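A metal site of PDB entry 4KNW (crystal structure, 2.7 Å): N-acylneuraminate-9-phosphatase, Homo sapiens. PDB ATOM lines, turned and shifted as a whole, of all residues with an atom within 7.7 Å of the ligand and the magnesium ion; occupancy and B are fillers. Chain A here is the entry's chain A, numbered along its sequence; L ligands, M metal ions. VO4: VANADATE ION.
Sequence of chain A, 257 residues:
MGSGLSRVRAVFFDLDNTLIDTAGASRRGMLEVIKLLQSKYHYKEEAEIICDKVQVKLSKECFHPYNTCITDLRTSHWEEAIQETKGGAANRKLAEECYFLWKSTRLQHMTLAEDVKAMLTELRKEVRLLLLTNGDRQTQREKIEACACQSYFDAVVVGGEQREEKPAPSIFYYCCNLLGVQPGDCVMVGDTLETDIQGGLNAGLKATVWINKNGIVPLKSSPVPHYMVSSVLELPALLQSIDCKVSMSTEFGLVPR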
ATOM      1  N   PHE A  13      21.411 -10.955  13.561  1.00  0.00           N
ATOM      2  CA  PHE A  13      21.157 -11.849  14.690  1.00  0.00           C
ATOM      3  C   PHE A  13      21.978 -13.124  14.600  1.00  0.00           C
ATOM      4  O   PHE A  13      21.958 -13.808  13.577  1.00  0.00           O
ATOM      5  CB  PHE A  13      19.682 -12.235  14.727  1.00  0.00           C
ATOM      6  CG  PHE A  13      18.791 -11.223  15.386  1.00  0.00           C
ATOM      7  CD1 PHE A  13      18.780 -11.081  16.769  1.00  0.00           C
ATOM      8  CD2 PHE A  13      17.940 -10.435  14.630  1.00  0.00           C
ATOM      9  CE1 PHE A  13      17.944 -10.167  17.378  1.00  0.00           C
ATOM     10  CE2 PHE A  13      17.100  -9.512  15.241  1.00  0.00           C
ATOM     11  CZ  PHE A  13      17.104  -9.383  16.614  1.00  0.00           C
ATOM     12  N   ASP A  14      22.695 -13.453  15.669  1.00  0.00           N
ATOM     13  CA  ASP A  14      23.319 -14.768  15.818  1.00  0.00           C
ATOM     14  C   ASP A  14      22.181 -15.765  16.042  1.00  0.00           C
ATOM     15  O   ASP A  14      21.090 -15.380  16.464  1.00  0.00           O
ATOM     16  CB  ASP A  14      24.280 -14.789  17.009  1.00  0.00           C
ATOM     17  CG  ASP A  14      24.967 -16.150  17.207  1.00  0.00           C
ATOM     18  OD1 ASP A  14      25.439 -16.746  16.218  1.00  0.00           O
ATOM     19  OD2 ASP A  14      25.040 -16.617  18.371  1.00  0.00           O
ATOM     20  N   LEU A  15      22.427 -17.045  15.760  1.00  0.00           N
ATOM     21  CA  LEU A  15      21.420 -18.068  15.989  1.00  0.00           C
ATOM     22  C   LEU A  15      21.659 -18.836  17.299  1.00  0.00           C
ATOM     23  O   LEU A  15      20.843 -18.751  18.233  1.00  0.00           O
ATOM     24  CB  LEU A  15      21.346 -19.032  14.805  1.00  0.00           C
ATOM     25  CG  LEU A  15      20.351 -20.203  14.899  1.00  0.00           C
ATOM     26  CD1 LEU A  15      18.919 -19.708  15.002  1.00  0.00           C
ATOM     27  CD2 LEU A  15      20.517 -21.122  13.711  1.00  0.00           C
ATOM     28  N   ASP A  16      22.779 -19.556  17.382  1.00  0.00           N
ATOM     29  CA  ASP A  16      23.036 -20.429  18.530  1.00  0.00           C
ATOM     30  C   ASP A  16      23.224 -19.686  19.847  1.00  0.00           C
ATOM     31  O   ASP A  16      24.100 -18.820  19.970  1.00  0.00           O
ATOM     32  CB  ASP A  16      24.257 -21.321  18.271  1.00  0.00           C
ATOM     33  CG  ASP A  16      24.131 -22.120  16.993  1.00  0.00           C
ATOM     34  OD1 ASP A  16      23.510 -23.205  17.008  1.00  0.00           O
ATOM     35  OD2 ASP A  16      24.683 -21.656  15.969  1.00  0.00           O
ATOM     36  N   ASN A  17      22.427 -20.064  20.841  1.00  0.00           N
ATOM     37  CA  ASN A  17      22.471 -19.471  22.185  1.00  0.00           C
ATOM     38  C   ASN A  17      22.135 -17.994  22.190  1.00  0.00           C
ATOM     39  O   ASN A  17      22.384 -17.296  23.172  1.00  0.00           O
ATOM     40  CB  ASN A  17      23.804 -19.759  22.903  1.00  0.00           C
ATOM     41  CG  ASN A  17      24.171 -21.229  22.885  1.00  0.00           C
ATOM     42  OD1 ASN A  17      23.491 -22.061  23.502  1.00  0.00           O
ATOM     43  ND2 ASN A  17      25.243 -21.563  22.185  1.00  0.00           N
ATOM     44  N   THR A  18      21.550 -17.521  21.092  1.00  0.00           N
ATOM     45  CA  THR A  18      21.056 -16.160  20.987  1.00  0.00           C
ATOM     46  C   THR A  18      19.561 -16.190  20.713  1.00  0.00           C
ATOM     47  O   THR A  18      18.782 -15.529  21.403  1.00  0.00           O
ATOM     48  CB  THR A  18      21.746 -15.393  19.848  1.00  0.00           C
ATOM     49  OG1 THR A  18      23.156 -15.340  20.081  1.00  0.00           O
ATOM     50  CG2 THR A  18      21.201 -13.981  19.760  1.00  0.00           C
ATOM     51  N   LEU A  19      19.170 -16.983  19.720  1.00  0.00           N
ATOM     52  CA  LEU A  19      17.763 -17.124  19.372  1.00  0.00           C
ATOM     53  C   LEU A  19      17.235 -18.504  19.757  1.00  0.00           C
ATOM     54  O   LEU A  19      16.053 -18.658  20.059  1.00  0.00           O
ATOM     55  CB  LEU A  19      17.558 -16.873  17.878  1.00  0.00           C
ATOM     56  CG  LEU A  19      17.689 -15.412  17.443  1.00  0.00           C
ATOM     57  CD1 LEU A  19      17.622 -15.292  15.930  1.00  0.00           C
ATOM     58  CD2 LEU A  19      16.616 -14.566  18.110  1.00  0.00           C
ATOM     59  N   ILE A  20      18.127 -19.496  19.749  1.00  0.00           N
ATOM     60  CA  ILE A  20      17.763 -20.838  20.190  1.00  0.00           C
ATOM     61  C   ILE A  20      18.719 -21.362  21.250  1.00  0.00           C
ATOM     62  O   ILE A  20      19.915 -21.046  21.241  1.00  0.00           O
ATOM     63  CB  ILE A  20      17.712 -21.839  19.021  1.00  0.00           C
ATOM     64  CG1 ILE A  20      19.082 -21.942  18.338  1.00  0.00           C
ATOM     65  CG2 ILE A  20      16.642 -21.455  18.013  1.00  0.00           C
ATOM     66  CD1 ILE A  20      19.114 -22.899  17.160  1.00  0.00           C
ATOM     67  N   THR A  22      20.835 -23.702  21.930  1.00  0.00           N
ATOM     68  CA  THR A  22      21.653 -24.775  21.378  1.00  0.00           C
ATOM     69  C   THR A  22      22.334 -25.589  22.479  1.00  0.00           C
ATOM     70  O   THR A  22      22.349 -26.823  22.434  1.00  0.00           O
ATOM     71  CB  THR A  22      22.724 -24.239  20.421  1.00  0.00           C
ATOM     72  OG1 THR A  22      22.098 -23.418  19.417  1.00  0.00           O
ATOM     73  CG2 THR A  22      23.468 -25.379  19.735  1.00  0.00           C
ATOM     74  N   LEU A 131      19.934 -12.920   9.595  1.00  0.00           N
ATOM     75  CA  LEU A 131      20.435 -13.990  10.436  1.00  0.00           C
ATOM     76  C   LEU A 131      21.871 -14.331  10.056  1.00  0.00           C
ATOM     77  O   LEU A 131      22.135 -14.830   8.967  1.00  0.00           O
ATOM     78  CB  LEU A 131      19.545 -15.229  10.306  1.00  0.00           C
ATOM     79  CG  LEU A 131      19.889 -16.416  11.203  1.00  0.00           C
ATOM     80  CD1 LEU A 131      19.742 -16.054  12.676  1.00  0.00           C
ATOM     81  CD2 LEU A 131      19.033 -17.614  10.858  1.00  0.00           C
ATOM     82  N   LEU A 132      22.796 -14.032  10.956  1.00  0.00           N
ATOM     83  CA  LEU A 132      24.213 -14.227  10.704  1.00  0.00           C
ATOM     84  C   LEU A 132      24.815 -15.246  11.662  1.00  0.00           C
ATOM     85  O   LEU A 132      24.991 -14.975  12.847  1.00  0.00           O
ATOM     86  CB  LEU A 132      24.959 -12.898  10.815  1.00  0.00           C
ATOM     87  CG  LEU A 132      26.469 -12.937  10.601  1.00  0.00           C
ATOM     88  CD1 LEU A 132      26.803 -13.666   9.309  1.00  0.00           C
ATOM     89  CD2 LEU A 132      27.027 -11.529  10.586  1.00  0.00           C
ATOM     90  N   THR A 133      25.130 -16.415  11.138  1.00  0.00           N
ATOM     91  CA  THR A 133      25.577 -17.530  11.953  1.00  0.00           C
ATOM     92  C   THR A 133      26.790 -18.223  11.340  1.00  0.00           C
ATOM     93  O   THR A 133      26.844 -18.438  10.130  1.00  0.00           O
ATOM     94  CB  THR A 133      24.442 -18.543  12.152  1.00  0.00           C
ATOM     95  OG1 THR A 133      24.967 -19.757  12.706  1.00  0.00           O
ATOM     96  CG2 THR A 133      23.769 -18.859  10.826  1.00  0.00           C
ATOM     97  N   ASN A 134      27.762 -18.554  12.184  1.00  0.00           N
ATOM     98  CA  ASN A 134      28.932 -19.308  11.745  1.00  0.00           C
ATOM     99  C   ASN A 134      28.614 -20.783  11.750  1.00  0.00           C
ATOM    100  O   ASN A 134      27.569 -21.205  12.241  1.00  0.00           O
ATOM    101  CB  ASN A 134      30.108 -19.052  12.701  1.00  0.00           C
ATOM    102  CG  ASN A 134      30.755 -17.700  12.472  1.00  0.00           C
ATOM    103  OD1 ASN A 134      30.239 -16.857  11.738  1.00  0.00           O
ATOM    104  ND2 ASN A 134      31.899 -17.494  13.104  1.00  0.00           N
ATOM    105  N   GLY A 135      29.526 -21.581  11.214  1.00  0.00           N
ATOM    106  CA  GLY A 135      29.331 -23.019  11.180  1.00  0.00           C
ATOM    107  C   GLY A 135      29.214 -23.555   9.768  1.00  0.00           C
ATOM    108  O   GLY A 135      29.023 -22.795   8.821  1.00  0.00           O
ATOM    109  N   GLN A 140      24.325 -26.087  10.171  1.00  0.00           N
ATOM    110  CA  GLN A 140      23.568 -24.866  10.454  1.00  0.00           C
ATOM    111  C   GLN A 140      22.216 -24.820   9.745  1.00  0.00           C
ATOM    112  O   GLN A 140      21.206 -24.495  10.373  1.00  0.00           O
ATOM    113  CB  GLN A 140      24.393 -23.611  10.143  1.00  0.00           C
ATOM    114  CG  GLN A 140      25.685 -23.514  10.950  1.00  0.00           C
ATOM    115  CD  GLN A 140      25.446 -23.654  12.450  1.00  0.00           C
ATOM    116  OE1 GLN A 140      25.911 -24.604  13.078  1.00  0.00           O
ATOM    117  NE2 GLN A 140      24.721 -22.699  13.028  1.00  0.00           N
ATOM    118  N   LYS A 143      19.672 -26.710  11.502  1.00  0.00           N
ATOM    119  CA  LYS A 143      19.159 -26.001  12.668  1.00  0.00           C
ATOM    120  C   LYS A 143      18.105 -24.980  12.258  1.00  0.00           C
ATOM    121  O   LYS A 143      17.057 -24.871  12.892  1.00  0.00           O
ATOM    122  CB  LYS A 143      20.280 -25.279  13.411  1.00  0.00           C
ATOM    123  CG  LYS A 143      21.348 -26.175  14.018  1.00  0.00           C
ATOM    124  CD  LYS A 143      22.371 -25.327  14.736  1.00  0.00           C
ATOM    125  CE  LYS A 143      23.576 -26.118  15.189  1.00  0.00           C
ATOM    126  NZ  LYS A 143      24.554 -25.213  15.854  1.00  0.00           N
ATOM    127  N   VAL A 157      22.462 -15.782   6.411  1.00  0.00           N
ATOM    128  CA  VAL A 157      23.819 -15.980   5.924  1.00  0.00           C
ATOM    129  C   VAL A 157      24.588 -16.934   6.829  1.00  0.00           C
ATOM    130  O   VAL A 157      24.781 -16.666   8.014  1.00  0.00           O
ATOM    131  CB  VAL A 157      24.588 -14.641   5.834  1.00  0.00           C
ATOM    132  CG1 VAL A 157      26.042 -14.899   5.488  1.00  0.00           C
ATOM    133  CG2 VAL A 157      23.935 -13.725   4.808  1.00  0.00           C
ATOM    134  N   GLY A 159      28.093 -18.887   7.680  1.00  0.00           N
ATOM    135  CA  GLY A 159      29.518 -18.712   7.492  1.00  0.00           C
ATOM    136  C   GLY A 159      30.232 -19.770   6.672  1.00  0.00           C
ATOM    137  O   GLY A 159      31.136 -19.465   5.903  1.00  0.00           O
ATOM    138  N   GLU A 165      34.030 -16.281   7.919  1.00  0.00           N
ATOM    139  CA  GLU A 165      33.023 -16.149   8.967  1.00  0.00           C
ATOM    140  C   GLU A 165      33.363 -14.989   9.890  1.00  0.00           C
ATOM    141  O   GLU A 165      34.306 -14.248   9.638  1.00  0.00           O
ATOM    142  CB  GLU A 165      32.958 -17.414   9.827  1.00  0.00           C
ATOM    143  CG  GLU A 165      32.613 -18.690   9.108  1.00  0.00           C
ATOM    144  CD  GLU A 165      32.444 -19.838  10.079  1.00  0.00           C
ATOM    145  OE1 GLU A 165      33.179 -19.881  11.092  1.00  0.00           O
ATOM    146  OE2 GLU A 165      31.554 -20.676   9.846  1.00  0.00           O
ATOM    147  N   LYS A 166      32.590 -14.854  10.960  1.00  0.00           N
ATOM    148  CA  LYS A 166      32.906 -13.907  12.009  1.00  0.00           C
ATOM    149  C   LYS A 166      34.167 -14.373  12.742  1.00  0.00           C
ATOM    150  O   LYS A 166      34.405 -15.570  12.849  1.00  0.00           O
ATOM    151  CB  LYS A 166      31.708 -13.797  12.966  1.00  0.00           C
ATOM    152  CG  LYS A 166      30.426 -13.361  12.269  1.00  0.00           C
ATOM    153  CD  LYS A 166      29.230 -13.361  13.208  1.00  0.00           C
ATOM    154  CE  LYS A 166      28.825 -14.771  13.604  1.00  0.00           C
ATOM    155  NZ  LYS A 166      27.585 -14.790  14.415  1.00  0.00           N
ATOM    156  N   MET A 188      24.687  -5.495  15.583  1.00  0.00           N
ATOM    157  CA  MET A 188      24.936  -6.933  15.664  1.00  0.00           C
ATOM    158  C   MET A 188      24.570  -7.457  17.043  1.00  0.00           C
ATOM    159  O   MET A 188      24.990  -6.908  18.060  1.00  0.00           O
ATOM    160  CB  MET A 188      26.386  -7.257  15.347  1.00  0.00           C
ATOM    161  CG  MET A 188      26.742  -8.727  15.517  1.00  0.00           C
ATOM    162  SD  MET A 188      25.799  -9.808  14.421  1.00  0.00           S
ATOM    163  CE  MET A 188      26.470 -11.411  14.846  1.00  0.00           C
ATOM    164  N   VAL A 189      23.761  -8.507  17.082  1.00  0.00           N
ATOM    165  CA  VAL A 189      23.336  -9.105  18.341  1.00  0.00           C
ATOM    166  C   VAL A 189      23.746 -10.564  18.429  1.00  0.00           C
ATOM    167  O   VAL A 189      23.393 -11.378  17.577  1.00  0.00           O
ATOM    168  CB  VAL A 189      21.817  -9.006  18.524  1.00  0.00           C
ATOM    169  CG1 VAL A 189      21.404  -9.645  19.846  1.00  0.00           C
ATOM    170  CG2 VAL A 189      21.371  -7.561  18.468  1.00  0.00           C
ATOM    171  N   GLY A 190      24.517 -10.881  19.466  1.00  0.00           N
ATOM    172  CA  GLY A 190      25.057 -12.211  19.645  1.00  0.00           C
ATOM    173  C   GLY A 190      25.584 -12.412  21.044  1.00  0.00           C
ATOM    174  O   GLY A 190      25.648 -11.460  21.839  1.00  0.00           O
ATOM    175  N   ASP A 191      25.983 -13.637  21.352  1.00  0.00           N
ATOM    176  CA  ASP A 191      26.315 -14.013  22.720  1.00  0.00           C
ATOM    177  C   ASP A 191      27.785 -14.379  22.857  1.00  0.00           C
ATOM    178  O   ASP A 191      28.242 -14.732  23.943  1.00  0.00           O
ATOM    179  CB  ASP A 191      25.459 -15.203  23.132  1.00  0.00           C
ATOM    180  CG  ASP A 191      25.768 -16.439  22.317  1.00  0.00           C
ATOM    181  OD1 ASP A 191      25.484 -16.449  21.102  1.00  0.00           O
ATOM    182  OD2 ASP A 191      26.324 -17.398  22.888  1.00  0.00           O
ATOM    183  N   THR A 192      28.529 -14.316  21.760  1.00  0.00           N
ATOM    184  CA  THR A 192      29.953 -14.594  21.801  1.00  0.00           C
ATOM    185  C   THR A 192      30.760 -13.349  21.494  1.00  0.00           C
ATOM    186  O   THR A 192      30.557 -12.703  20.462  1.00  0.00           O
ATOM    187  CB  THR A 192      30.348 -15.714  20.820  1.00  0.00           C
ATOM    188  OG1 THR A 192      29.811 -16.956  21.287  1.00  0.00           O
ATOM    189  CG2 THR A 192      31.839 -15.847  20.729  1.00  0.00           C
ATOM    190  N   THR A 195      33.394 -13.518  18.327  1.00  0.00           N
ATOM    191  CA  THR A 195      32.858 -13.572  16.971  1.00  0.00           C
ATOM    192  C   THR A 195      31.856 -12.443  16.718  1.00  0.00           C
ATOM    193  O   THR A 195      32.128 -11.515  15.952  1.00  0.00           O
ATOM    194  CB  THR A 195      32.167 -14.919  16.705  1.00  0.00           C
ATOM    195  OG1 THR A 195      31.057 -15.082  17.595  1.00  0.00           O
ATOM    196  CG2 THR A 195      33.131 -16.070  16.916  1.00  0.00           C
ATOM    197  N   ASP A 196      30.696 -12.542  17.352  1.00  0.00           N
ATOM    198  CA  ASP A 196      29.618 -11.570  17.162  1.00  0.00           C
ATOM    199  C   ASP A 196      30.053 -10.141  17.497  1.00  0.00           C
ATOM    200  O   ASP A 196      29.801  -9.211  16.732  1.00  0.00           O
ATOM    201  CB  ASP A 196      28.394 -11.954  18.004  1.00  0.00           C
ATOM    202  CG  ASP A 196      28.003 -13.403  17.818  1.00  0.00           C
ATOM    203  OD1 ASP A 196      28.047 -13.889  16.669  1.00  0.00           O
ATOM    204  OD2 ASP A 196      27.653 -14.077  18.814  1.00  0.00           O
ATOM    205  N   ILE A 211      24.856 -10.768  24.424  1.00  0.00           N
ATOM    206  CA  ILE A 211      23.891 -11.528  25.187  1.00  0.00           C
ATOM    207  C   ILE A 211      24.608 -12.328  26.256  1.00  0.00           C
ATOM    208  O   ILE A 211      25.363 -13.247  25.956  1.00  0.00           O
ATOM    209  CB  ILE A 211      23.090 -12.486  24.289  1.00  0.00           C
ATOM    210  CG1 ILE A 211      22.469 -11.740  23.116  1.00  0.00           C
ATOM    211  CG2 ILE A 211      22.030 -13.215  25.108  1.00  0.00           C
ATOM    212  CD1 ILE A 211      21.537 -10.636  23.519  1.00  0.00           C
HETATM  213  V   VO4 L   1      26.358 -18.653  15.992  1.00  0.00           V
HETATM  214  O1  VO4 L   1      27.243 -20.315  15.668  1.00  0.00           O
HETATM  215  O2  VO4 L   1      27.298 -17.271  15.053  1.00  0.00           O
HETATM  216  O3  VO4 L   1      26.339 -18.312  17.870  1.00  0.00           O
HETATM  217  O4  VO4 L   1      24.562 -18.741  15.362  1.00  0.00           O
HETATM  218 MG    MG M   1      25.977 -17.959  19.822  1.00  0.00          MG
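A vanadium atom (V) of the ligand is bound by the side-chain carboxylate (OD1) of Asp 14 (2.1 Å). An oxygen (O2) of the ligand sits close to the side-chain amino group (NZ) of Lys 166 (2.6 Å).
N of Thr 133 lies within hydrogen-bond range of O of Val 157. The side-chain hydroxyl of Thr 22 sits at hydrogen-bond distance from the side-chain carboxylate of Asp 16. The backbone carbonyl oxygen of Leu 15 sits at hydrogen-bond distance from the backbone NH of Ile 20 (3.2 Å). The backbone NH of Asp 191 is in hydrogen-bond range of the side-chain carboxylate of Asp 196 (3.1 Å). The side-chain carboxylate of Asp 16 sits at hydrogen-bond distance from the side-chain amide nitrogen of Gln 140 (3.1 Å). The side-chain carboxylate of Asp 16 lies within salt-bridge range of the side-chain amino group of Lys 143 (2.5 Å). ND2 of Asn 134 is in hydrogen-bond range of OE1 of Glu 165 (3.4 Å). The side-chain amide nitrogen (ND2) of Asn 134 is in hydrogen-bond range of the backbone carbonyl oxygen (O) of Lys 166 (3.2 Å).
O4 of the ligand lies close to N of Leu 15 (2.8 Å). The side-chain hydroxyl (OG1) of Thr 133 sits close to an oxygen (O4) of the ligand (2.9 Å). The backbone NH of Asn 134 sits close to an oxygen (O2) of the ligand (3.2 Å). Residues that only touch the ligand: Leu 132 (3.9 Å) and Asp 196 (3.8 Å). Hydrophobic or aromatic side chains within 4 Å of the ligand: Leu 15.
Residues that only touch the magnesium ion: Thr 18 (3.9 Å). The nearest printed residue that does not touch the magnesium ion is Asn 17 (4.2 Å).
The magnesium ion is bound by an oxygen (O3) of the ligand, the side-chain carboxylate (OD1) of Asp 191, the backbone carbonyl oxygen (O) of Asp 16 and the side-chain carboxylate (OD2) of Asp 14.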
